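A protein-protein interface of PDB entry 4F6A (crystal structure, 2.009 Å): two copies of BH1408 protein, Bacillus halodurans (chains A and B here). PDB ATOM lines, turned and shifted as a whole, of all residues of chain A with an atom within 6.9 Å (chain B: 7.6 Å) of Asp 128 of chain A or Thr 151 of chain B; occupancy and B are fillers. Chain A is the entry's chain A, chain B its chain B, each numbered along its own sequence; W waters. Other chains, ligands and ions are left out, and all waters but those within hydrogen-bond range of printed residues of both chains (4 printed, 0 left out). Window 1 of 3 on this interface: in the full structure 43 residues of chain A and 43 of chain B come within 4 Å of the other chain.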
ATOM      1  N   TYR A  90     -26.833   7.010  12.083  1.00  0.00           N
ATOM      2  CA  TYR A  90     -27.841   6.297  12.849  1.00  0.00           C
ATOM      3  C   TYR A  90     -28.560   5.300  11.941  1.00  0.00           C
ATOM      4  O   TYR A  90     -29.071   5.676  10.897  1.00  0.00           O
ATOM      5  CB  TYR A  90     -28.845   7.269  13.465  1.00  0.00           C
ATOM      6  CG  TYR A  90     -29.892   6.579  14.311  1.00  0.00           C
ATOM      7  CD1 TYR A  90     -29.612   6.181  15.616  1.00  0.00           C
ATOM      8  CD2 TYR A  90     -31.161   6.328  13.804  1.00  0.00           C
ATOM      9  CE1 TYR A  90     -30.576   5.546  16.393  1.00  0.00           C
ATOM     10  CE2 TYR A  90     -32.125   5.698  14.565  1.00  0.00           C
ATOM     11  CZ  TYR A  90     -31.832   5.310  15.851  1.00  0.00           C
ATOM     12  OH  TYR A  90     -32.805   4.691  16.593  1.00  0.00           O
ATOM     13  N   ILE A  91     -28.561   4.027  12.329  1.00  0.00           N
ATOM     14  CA  ILE A  91     -29.280   2.992  11.571  1.00  0.00           C
ATOM     15  C   ILE A  91     -30.703   2.854  12.118  1.00  0.00           C
ATOM     16  O   ILE A  91     -30.881   2.365  13.234  1.00  0.00           O
ATOM     17  CB  ILE A  91     -28.571   1.619  11.694  1.00  0.00           C
ATOM     18  CG1 ILE A  91     -27.105   1.732  11.257  1.00  0.00           C
ATOM     19  CG2 ILE A  91     -29.320   0.552  10.890  1.00  0.00           C
ATOM     20  CD1 ILE A  91     -26.268   0.448  11.517  1.00  0.00           C
ATOM     21  N   SER A  92     -31.705   3.298  11.354  1.00  0.00           N
ATOM     22  CA  SER A  92     -33.104   3.199  11.797  1.00  0.00           C
ATOM     23  C   SER A  92     -33.733   1.839  11.468  1.00  0.00           C
ATOM     24  O   SER A  92     -34.697   1.417  12.105  1.00  0.00           O
ATOM     25  CB  SER A  92     -33.963   4.331  11.210  1.00  0.00           C
ATOM     26  OG  SER A  92     -33.994   4.268   9.797  1.00  0.00           O
ATOM     27  N   GLU A 126     -24.609   4.419  15.422  1.00  0.00           N
ATOM     28  CA  GLU A 126     -25.522   4.146  16.521  1.00  0.00           C
ATOM     29  C   GLU A 126     -26.806   3.527  15.989  1.00  0.00           C
ATOM     30  O   GLU A 126     -27.152   3.701  14.820  1.00  0.00           O
ATOM     31  CB  GLU A 126     -25.836   5.439  17.295  1.00  0.00           C
ATOM     32  CG  GLU A 126     -24.607   6.047  17.986  1.00  0.00           C
ATOM     33  CD  GLU A 126     -24.921   7.338  18.742  1.00  0.00           C
ATOM     34  OE1 GLU A 126     -25.995   7.926  18.508  1.00  0.00           O
ATOM     35  OE2 GLU A 126     -24.092   7.757  19.576  1.00  0.00           O
ATOM     36  N   LEU A 127     -27.503   2.801  16.855  1.00  0.00           N
ATOM     37  CA  LEU A 127     -28.829   2.281  16.538  1.00  0.00           C
ATOM     38  C   LEU A 127     -29.564   1.993  17.840  1.00  0.00           C
ATOM     39  O   LEU A 127     -28.953   1.968  18.913  1.00  0.00           O
ATOM     40  CB  LEU A 127     -28.721   1.000  15.686  1.00  0.00           C
ATOM     41  CG  LEU A 127     -27.926  -0.198  16.224  1.00  0.00           C
ATOM     42  CD1 LEU A 127     -28.678  -1.049  17.274  1.00  0.00           C
ATOM     43  CD2 LEU A 127     -27.443  -1.088  15.055  1.00  0.00           C
ATOM     44  N   ASP A 128     -30.862   1.727  17.747  1.00  0.00           N
ATOM     45  CA  ASP A 128     -31.620   1.258  18.911  1.00  0.00           C
ATOM     46  C   ASP A 128     -32.204  -0.147  18.698  1.00  0.00           C
ATOM     47  O   ASP A 128     -32.685  -0.469  17.612  1.00  0.00           O
ATOM     48  CB  ASP A 128     -32.705   2.270  19.275  1.00  0.00           C
ATOM     49  CG  ASP A 128     -32.116   3.560  19.862  1.00  0.00           C
ATOM     50  OD1 ASP A 128     -31.943   4.542  19.113  1.00  0.00           O
ATOM     51  OD2 ASP A 128     -31.800   3.573  21.065  1.00  0.00           O
ATOM     52  N   VAL A 129     -32.172  -0.972  19.741  1.00  0.00           N
ATOM     53  CA  VAL A 129     -32.642  -2.353  19.651  1.00  0.00           C
ATOM     54  C   VAL A 129     -33.456  -2.728  20.898  1.00  0.00           C
ATOM     55  O   VAL A 129     -33.075  -2.393  22.024  1.00  0.00           O
ATOM     56  CB  VAL A 129     -31.443  -3.343  19.434  1.00  0.00           C
ATOM     57  CG1 VAL A 129     -30.410  -3.228  20.555  1.00  0.00           C
ATOM     58  CG2 VAL A 129     -31.916  -4.788  19.312  1.00  0.00           C
ATOM     59  N   TYR A 130     -34.583  -3.403  20.700  1.00  0.00           N
ATOM     60  CA  TYR A 130     -35.405  -3.822  21.838  1.00  0.00           C
ATOM     61  C   TYR A 130     -34.745  -4.938  22.628  1.00  0.00           C
ATOM     62  O   TYR A 130     -34.065  -5.798  22.061  1.00  0.00           O
ATOM     63  CB  TYR A 130     -36.831  -4.198  21.400  1.00  0.00           C
ATOM     64  CG  TYR A 130     -37.675  -2.967  21.211  1.00  0.00           C
ATOM     65  CD1 TYR A 130     -37.556  -2.198  20.064  1.00  0.00           C
ATOM     66  CD2 TYR A 130     -38.545  -2.530  22.211  1.00  0.00           C
ATOM     67  CE1 TYR A 130     -38.293  -1.036  19.904  1.00  0.00           C
ATOM     68  CE2 TYR A 130     -39.289  -1.369  22.056  1.00  0.00           C
ATOM     69  CZ  TYR A 130     -39.157  -0.633  20.896  1.00  0.00           C
ATOM     70  OH  TYR A 130     -39.874   0.521  20.714  1.00  0.00           O
ATOM     71  N   TYR A 140     -25.287  -7.428  16.474  1.00  0.00           N
ATOM     72  CA  TYR A 140     -24.556  -6.164  16.592  1.00  0.00           C
ATOM     73  C   TYR A 140     -23.351  -6.303  17.519  1.00  0.00           C
ATOM     74  O   TYR A 140     -22.290  -5.734  17.260  1.00  0.00           O
ATOM     75  CB  TYR A 140     -25.502  -5.023  17.000  1.00  0.00           C
ATOM     76  CG  TYR A 140     -26.465  -4.738  15.878  1.00  0.00           C
ATOM     77  CD1 TYR A 140     -25.984  -4.405  14.619  1.00  0.00           C
ATOM     78  CD2 TYR A 140     -27.839  -4.866  16.044  1.00  0.00           C
ATOM     79  CE1 TYR A 140     -26.836  -4.176  13.573  1.00  0.00           C
ATOM     80  CE2 TYR A 140     -28.709  -4.634  14.985  1.00  0.00           C
ATOM     81  CZ  TYR A 140     -28.187  -4.295  13.754  1.00  0.00           C
ATOM     82  OH  TYR A 140     -29.004  -4.058  12.676  1.00  0.00           O
ATOM     83  N   MET A 145     -20.323  -3.712  18.280  1.00  0.00           N
ATOM     84  CA  MET A 145     -21.136  -2.660  18.905  1.00  0.00           C
ATOM     85  C   MET A 145     -21.335  -2.955  20.397  1.00  0.00           C
ATOM     86  O   MET A 145     -21.392  -4.113  20.794  1.00  0.00           O
ATOM     87  CB  MET A 145     -22.503  -2.527  18.229  1.00  0.00           C
ATOM     88  CG  MET A 145     -22.452  -2.339  16.711  1.00  0.00           C
ATOM     89  SD  MET A 145     -24.127  -1.594  16.036  1.00  0.00           S
ATOM     90  CE  MET A 145     -23.877   0.281  16.651  1.00  0.00           C
ATOM     91  N   ARG A 146     -21.464  -1.908  21.209  1.00  0.00           N
ATOM     92  CA  ARG A 146     -21.679  -2.080  22.643  1.00  0.00           C
ATOM     93  C   ARG A 146     -22.785  -1.145  23.139  1.00  0.00           C
ATOM     94  O   ARG A 146     -23.113  -0.145  22.499  1.00  0.00           O
ATOM     95  CB  ARG A 146     -20.375  -1.845  23.420  1.00  0.00           C
ATOM     96  CG  ARG A 146     -19.233  -2.820  23.081  1.00  0.00           C
ATOM     97  CD  ARG A 146     -19.526  -4.233  23.553  1.00  0.00           C
ATOM     98  NE  ARG A 146     -18.399  -5.156  23.347  1.00  0.00           N
ATOM     99  CZ  ARG A 146     -18.239  -5.916  22.262  1.00  0.00           C
ATOM    100  NH1 ARG A 146     -19.123  -5.867  21.272  1.00  0.00           N
ATOM    101  NH2 ARG A 146     -17.193  -6.723  22.157  1.00  0.00           N
ATOM    102  N   CYS A 147     -23.368  -1.463  24.286  1.00  0.00           N
ATOM    103  CA  CYS A 147     -24.480  -0.660  24.799  1.00  0.00           C
ATOM    104  C   CYS A 147     -24.005   0.715  25.282  1.00  0.00           C
ATOM    105  O   CYS A 147     -23.082   0.798  26.085  1.00  0.00           O
ATOM    106  CB  CYS A 147     -25.181  -1.413  25.940  1.00  0.00           C
ATOM    107  SG  CYS A 147     -26.529  -0.451  26.691  1.00  0.00           S
ATOM    108  N   GLN A 148     -24.605   1.787  24.757  1.00  0.00           N
ATOM    109  CA  GLN A 148     -24.312   3.161  25.186  1.00  0.00           C
ATOM    110  C   GLN A 148     -25.208   3.579  26.351  1.00  0.00           C
ATOM    111  O   GLN A 148     -24.751   4.163  27.339  1.00  0.00           O
ATOM    112  CB  GLN A 148     -24.562   4.131  24.030  1.00  0.00           C
ATOM    113  CG  GLN A 148     -24.243   5.585  24.335  1.00  0.00           C
ATOM    114  CD  GLN A 148     -24.632   6.507  23.192  1.00  0.00           C
ATOM    115  OE1 GLN A 148     -25.723   7.074  23.178  1.00  0.00           O
ATOM    116  NE2 GLN A 148     -23.747   6.642  22.216  1.00  0.00           N
ATOM    117  N   LYS A 149     -26.495   3.286  26.205  1.00  0.00           N
ATOM    118  CA  LYS A 149     -27.516   3.690  27.159  1.00  0.00           C
ATOM    119  C   LYS A 149     -28.747   2.840  26.928  1.00  0.00           C
ATOM    120  O   LYS A 149     -28.876   2.189  25.883  1.00  0.00           O
ATOM    121  CB  LYS A 149     -27.879   5.178  27.012  1.00  0.00           C
ATOM    122  CG  LYS A 149     -28.265   5.656  25.614  1.00  0.00           C
ATOM    123  CD  LYS A 149     -28.738   7.129  25.665  1.00  0.00           C
ATOM    124  CE  LYS A 149     -28.969   7.723  24.277  1.00  0.00           C
ATOM    125  NZ  LYS A 149     -30.187   7.172  23.620  1.00  0.00           N
ATOM    126  N   GLN A 150     -29.652   2.840  27.900  1.00  0.00           N
ATOM    127  CA  GLN A 150     -30.854   2.036  27.780  1.00  0.00           C
ATOM    128  C   GLN A 150     -32.077   2.749  28.311  1.00  0.00           C
ATOM    129  O   GLN A 150     -31.987   3.614  29.193  1.00  0.00           O
ATOM    130  CB  GLN A 150     -30.674   0.669  28.456  1.00  0.00           C
ATOM    131  CG  GLN A 150     -30.312   0.706  29.922  1.00  0.00           C
ATOM    132  CD  GLN A 150     -29.948  -0.681  30.474  1.00  0.00           C
ATOM    133  OE1 GLN A 150     -30.748  -1.314  31.155  1.00  0.00           O
ATOM    134  NE2 GLN A 150     -28.743  -1.145  30.177  1.00  0.00           N
ATOM    135  N   THR A 151     -33.221   2.387  27.740  1.00  0.00           N
ATOM    136  CA  THR A 151     -34.513   2.872  28.180  1.00  0.00           C
ATOM    137  C   THR A 151     -35.027   1.845  29.158  1.00  0.00           C
ATOM    138  O   THR A 151     -35.051   0.639  28.862  1.00  0.00           O
ATOM    139  CB  THR A 151     -35.512   2.967  27.007  1.00  0.00           C
ATOM    140  OG1 THR A 151     -34.974   3.813  25.976  1.00  0.00           O
ATOM    141  CG2 THR A 151     -36.867   3.530  27.496  1.00  0.00           C
ATOM    142  N   ASP B 128     -34.302   7.033  30.588  1.00  0.00           N
ATOM    143  CA  ASP B 128     -33.073   6.584  29.936  1.00  0.00           C
ATOM    144  C   ASP B 128     -31.872   6.741  30.874  1.00  0.00           C
ATOM    145  O   ASP B 128     -31.778   7.724  31.602  1.00  0.00           O
ATOM    146  CB  ASP B 128     -32.873   7.370  28.632  1.00  0.00           C
ATOM    147  CG  ASP B 128     -33.854   6.937  27.552  1.00  0.00           C
ATOM    148  OD1 ASP B 128     -34.797   7.693  27.254  1.00  0.00           O
ATOM    149  OD2 ASP B 128     -33.696   5.817  27.030  1.00  0.00           O
ATOM    150  N   VAL B 129     -30.967   5.765  30.871  1.00  0.00           N
ATOM    151  CA  VAL B 129     -29.812   5.782  31.752  1.00  0.00           C
ATOM    152  C   VAL B 129     -28.596   5.266  30.990  1.00  0.00           C
ATOM    153  O   VAL B 129     -28.700   4.304  30.230  1.00  0.00           O
ATOM    154  CB  VAL B 129     -30.062   4.940  33.039  1.00  0.00           C
ATOM    155  CG1 VAL B 129     -30.523   3.508  32.698  1.00  0.00           C
ATOM    156  CG2 VAL B 129     -28.824   4.908  33.931  1.00  0.00           C
ATOM    157  N   ASP B 131     -25.092   3.414  30.080  1.00  0.00           N
ATOM    158  CA  ASP B 131     -24.644   2.079  30.453  1.00  0.00           C
ATOM    159  C   ASP B 131     -23.529   2.094  31.500  1.00  0.00           C
ATOM    160  O   ASP B 131     -23.409   1.157  32.299  1.00  0.00           O
ATOM    161  CB  ASP B 131     -24.221   1.267  29.216  1.00  0.00           C
ATOM    162  CG  ASP B 131     -24.013  -0.201  29.532  1.00  0.00           C
ATOM    163  OD1 ASP B 131     -24.995  -0.874  29.920  1.00  0.00           O
ATOM    164  OD2 ASP B 131     -22.873  -0.678  29.381  1.00  0.00           O
ATOM    165  N   CYS B 147     -35.086  -3.207  31.567  1.00  0.00           N
ATOM    166  CA  CYS B 147     -34.676  -2.687  30.271  1.00  0.00           C
ATOM    167  C   CYS B 147     -35.733  -2.946  29.187  1.00  0.00           C
ATOM    168  O   CYS B 147     -36.131  -4.090  28.946  1.00  0.00           O
ATOM    169  CB  CYS B 147     -33.344  -3.305  29.845  1.00  0.00           C
ATOM    170  SG  CYS B 147     -32.778  -2.668  28.247  1.00  0.00           S
ATOM    171  N   LYS B 149     -35.370  -1.223  25.912  1.00  0.00           N
ATOM    172  CA  LYS B 149     -34.572  -1.194  24.699  1.00  0.00           C
ATOM    173  C   LYS B 149     -33.268  -0.478  25.009  1.00  0.00           C
ATOM    174  O   LYS B 149     -33.138   0.164  26.057  1.00  0.00           O
ATOM    175  CB  LYS B 149     -35.314  -0.464  23.558  1.00  0.00           C
ATOM    176  CG  LYS B 149     -35.833   0.932  23.890  1.00  0.00           C
ATOM    177  CD  LYS B 149     -36.634   1.526  22.707  1.00  0.00           C
ATOM    178  CE  LYS B 149     -37.185   2.919  23.001  1.00  0.00           C
ATOM    179  NZ  LYS B 149     -36.098   3.900  23.270  1.00  0.00           N
ATOM    180  N   GLN B 150     -32.306  -0.581  24.097  1.00  0.00           N
ATOM    181  CA  GLN B 150     -31.018   0.063  24.302  1.00  0.00           C
ATOM    182  C   GLN B 150     -30.435   0.667  23.035  1.00  0.00           C
ATOM    183  O   GLN B 150     -30.699   0.207  21.914  1.00  0.00           O
ATOM    184  CB  GLN B 150     -30.011  -0.900  24.942  1.00  0.00           C
ATOM    185  CG  GLN B 150     -29.842  -2.252  24.245  1.00  0.00           C
ATOM    186  CD  GLN B 150     -28.920  -3.212  25.022  1.00  0.00           C
ATOM    187  OE1 GLN B 150     -27.697  -3.089  24.977  1.00  0.00           O
ATOM    188  NE2 GLN B 150     -29.513  -4.166  25.732  1.00  0.00           N
ATOM    189  N   THR B 151     -29.640   1.707  23.239  1.00  0.00           N
ATOM    190  CA  THR B 151     -28.864   2.329  22.180  1.00  0.00           C
ATOM    191  C   THR B 151     -27.501   1.658  22.148  1.00  0.00           C
ATOM    192  O   THR B 151     -26.833   1.510  23.182  1.00  0.00           O
ATOM    193  CB  THR B 151     -28.688   3.853  22.434  1.00  0.00           C
ATOM    194  OG1 THR B 151     -29.971   4.451  22.680  1.00  0.00           O
ATOM    195  CG2 THR B 151     -28.036   4.538  21.225  1.00  0.00           C
ATOM    196  N   MET B 152     -27.100   1.212  20.965  1.00  0.00           N
ATOM    197  CA  MET B 152     -25.785   0.627  20.790  1.00  0.00           C
ATOM    198  C   MET B 152     -24.943   1.537  19.956  1.00  0.00           C
ATOM    199  O   MET B 152     -25.471   2.318  19.176  1.00  0.00           O
ATOM    200  CB  MET B 152     -25.938  -0.701  20.087  1.00  0.00           C
ATOM    201  CG  MET B 152     -27.065  -1.380  20.718  1.00  0.00           C
ATOM    202  SD  MET B 152     -26.323  -2.840  21.620  1.00  0.00           S
ATOM    203  CE  MET B 152     -26.823  -3.872  20.136  1.00  0.00           C
ATOM    204  N   GLU B 153     -23.628   1.439  20.130  1.00  0.00           N
ATOM    205  CA  GLU B 153     -22.743   2.401  19.502  1.00  0.00           C
ATOM    206  C   GLU B 153     -21.483   1.682  19.045  1.00  0.00           C
ATOM    207  O   GLU B 153     -21.078   0.686  19.639  1.00  0.00           O
ATOM    208  CB  GLU B 153     -22.391   3.522  20.487  1.00  0.00           C
ATOM    209  CG  GLU B 153     -21.500   3.039  21.651  1.00  0.00           C
ATOM    210  CD  GLU B 153     -21.272   4.116  22.709  1.00  0.00           C
ATOM    211  OE1 GLU B 153     -21.360   5.318  22.380  1.00  0.00           O
ATOM    212  OE2 GLU B 153     -21.009   3.753  23.874  1.00  0.00           O
HETATM  213  O   HOH W   1     -22.310   4.676  28.652  1.00  0.00           O
HETATM  214  O   HOH W   2     -32.297   9.233  25.353  1.00  0.00           O
HETATM  215  O   HOH W   3     -31.752   4.717  25.279  1.00  0.00           O
HETATM  216  O   HOH W   4     -20.526   1.554  25.287  1.00  0.00           O
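The side-chain sulfur (SG) of Cys 147 of chain A sits at hydrogen-bond distance from the side-chain carboxylate (OD1) of Asp 131 of chain B. OE1 of Glu 153 of chain B is in hydrogen-bond range of NE2 of Gln 148 of chain A, at 2.7 Å. N of Gln 150 of chain B is in hydrogen-bond range of O of Val 129 of chain A, at 2.9 Å. OE1 of Gln 150 of chain A lies close to SG of Cys 147 of chain B (3.8 Å). The backbone carbonyl oxygen (O) of Gln 148 of chain A sits at hydrogen-bond distance from the backbone NH (N) of Asp 131 of chain B (2.9 Å). OG1 of Thr 151 of chain A sits at hydrogen-bond distance from OD2 of Asp 128 of chain B. The backbone NH of Gln 148 of chain A lies within hydrogen-bond range of the backbone carbonyl oxygen of Thr 151 of chain B (2.7 Å). The backbone NH (N) of Thr 151 of chain A lies within hydrogen-bond range of the backbone carbonyl oxygen (O) of Lys 149 of chain B, 2.8 Å away. The side-chain sulfur (SG) of Cys 147 of chain A sits close to the side-chain amide oxygen (OE1) of Gln 150 of chain B (3.4 Å). O of Val 129 of chain B sits at hydrogen-bond distance from N of Gln 150 of chain A, 2.9 Å away. The backbone carbonyl oxygen of Leu 127 of chain A sits at hydrogen-bond distance from the backbone NH of Met 152 of chain B. The backbone carbonyl oxygen (O) of Arg 146 of chain A is in hydrogen-bond range of the backbone NH (N) of Glu 153 of chain B, at 2.9 Å. The backbone carbonyl oxygen (O) of Lys 149 of chain A sits at hydrogen-bond distance from the backbone NH (N) of Thr 151 of chain B, 2.8 Å away. OD2 of Asp 128 of chain A is in hydrogen-bond range of OG1 of Thr 151 of chain B (2.6 Å).
Cys 147 of chain A touches Gln 150 of chain B, and with the chains exchanged Gln 150 of chain A touches Cys 147 of chain B. Cys 147 of chain A touches Thr 151 of chain B, and with the chains exchanged Thr 151 of chain A touches Cys 147 of chain B. Lys 149 of chain A touches Gln 150 of chain B, and with the chains exchanged Gln 150 of chain A touches Lys 149 of chain B. Gln 150 of chain B touches its own counterpart, Gln 150 of chain A. Of the 34 pairs that touch across the chains among the printed residues, 17 have their exchanged pair printed and touching as well.
Hydrophobic or aromatic side chains of chain B within 4 Å of the printed part of chain A: Val 129 and Met 152.
Asp 128 of chain A touches just these residues of chain B: Gln 150 and Thr 151. Thr 151 of chain B touches five residues of chain A. Of the printed residues of chain B, Val 129 of chain A touches Lys 149, Gln 150 and Met 152. Of the printed residues of chain A, Gln 150 of chain B touches Leu 127 (3.9 Å), Asp 128 (3.3 Å), Val 129 (2.9 Å), Cys 147 (3.2 Å), Lys 149 (3.4 Å) and Gln 150 (3.9 Å). Ser 92 of chain A touches none of the printed residues of chain B. Tyr 90 of chain A touches none of the printed residues of chain B. The nearest residue of chain A that does not touch Thr 151 of chain B is Arg 146 of chain A (4.1 Å). The nearest printed residue of chain B that does not touch Arg 146 of chain A is Thr 151 of chain B (4.1 Å).
Water W4 lies within hydrogen-bond range of OE2 of Glu 153 of chain B and O of Cys 147 of chain A. Water W1 lies within hydrogen-bond range of the backbone carbonyl oxygen of Gln 148 of chain A (2.8 Å) and the backbone NH of Asp 131 of chain B (3.4 Å). Water W3 lies within hydrogen-bond range of the side-chain carboxylate (OD2) of Asp 128 of chain B (2.8 Å), the side-chain hydroxyl (OG1) of Thr 151 of chain B (3.2 Å), the side-chain amino group (NZ) of Lys 149 of chain A (3.4 Å) and the side-chain hydroxyl (OG1) of Thr 151 of chain A (3.4 Å). Water W2 bridges the side-chain amino group (NZ) of Lys 149 of chain A and the side-chain carboxylate (OD1) of Asp 128 of chain B.
Among the printed residues, merely in contact across the chains: Glu 126 of chain A with Met 152 of chain B, Leu 127 of chain A with Gln 150 of chain B, Leu 127 of chain A with Thr 151 of chain B, Asp 128 of chain A with Gln 150 of chain B, Val 129 of chain A with Lys 149 of chain B, Val 129 of chain A with Met 152 of chain B, Tyr 130 of chain A with Lys 149 of chain B, Tyr 140 of chain A with Met 152 of chain B, Met 145 of chain A with Met 152 of chain B, Met 145 of chain A with Glu 153 of chain B, Arg 146 of chain A with Met 152 of chain B, Cys 147 of chain A with Thr 151 of chain B, Lys 149 of chain A with Val 129 of chain B, Lys 149 of chain A with Asp 131 of chain B, Lys 149 of chain A with Gln 150 of chain B, Gln 150 of chain A with Asp 128 of chain B, Gln 150 of chain A with Asp 131 of chain B, Gln 150 of chain A with Lys 149 of chain B, Gln 150 of chain A with Gln 150 of chain B and Thr 151 of chain A with Cys 147 of chain B.
The side-chain carboxylate of Glu 126 of chain A is in hydrogen-bond range of the side-chain amide nitrogen of Gln 148 of chain A (2.9 Å). N of Met 145 of chain A is in hydrogen-bond range of O of Tyr 140 of chain A. O of Lys 149 of chain B is in hydrogen-bond range of SG of Cys 147 of chain B (3.6 Å). The side-chain amide oxygen of Gln 150 of chain B sits close to the side-chain sulfur of Met 152 of chain B (3.6 Å). The backbone NH of Ile 91 of chain A is in hydrogen-bond range of the backbone carbonyl oxygen of Glu 126 of chain A (2.9 Å). OD1 of Asp 128 of chain A sits at hydrogen-bond distance from OH of Tyr 90 of chain A, 2.7 Å away.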
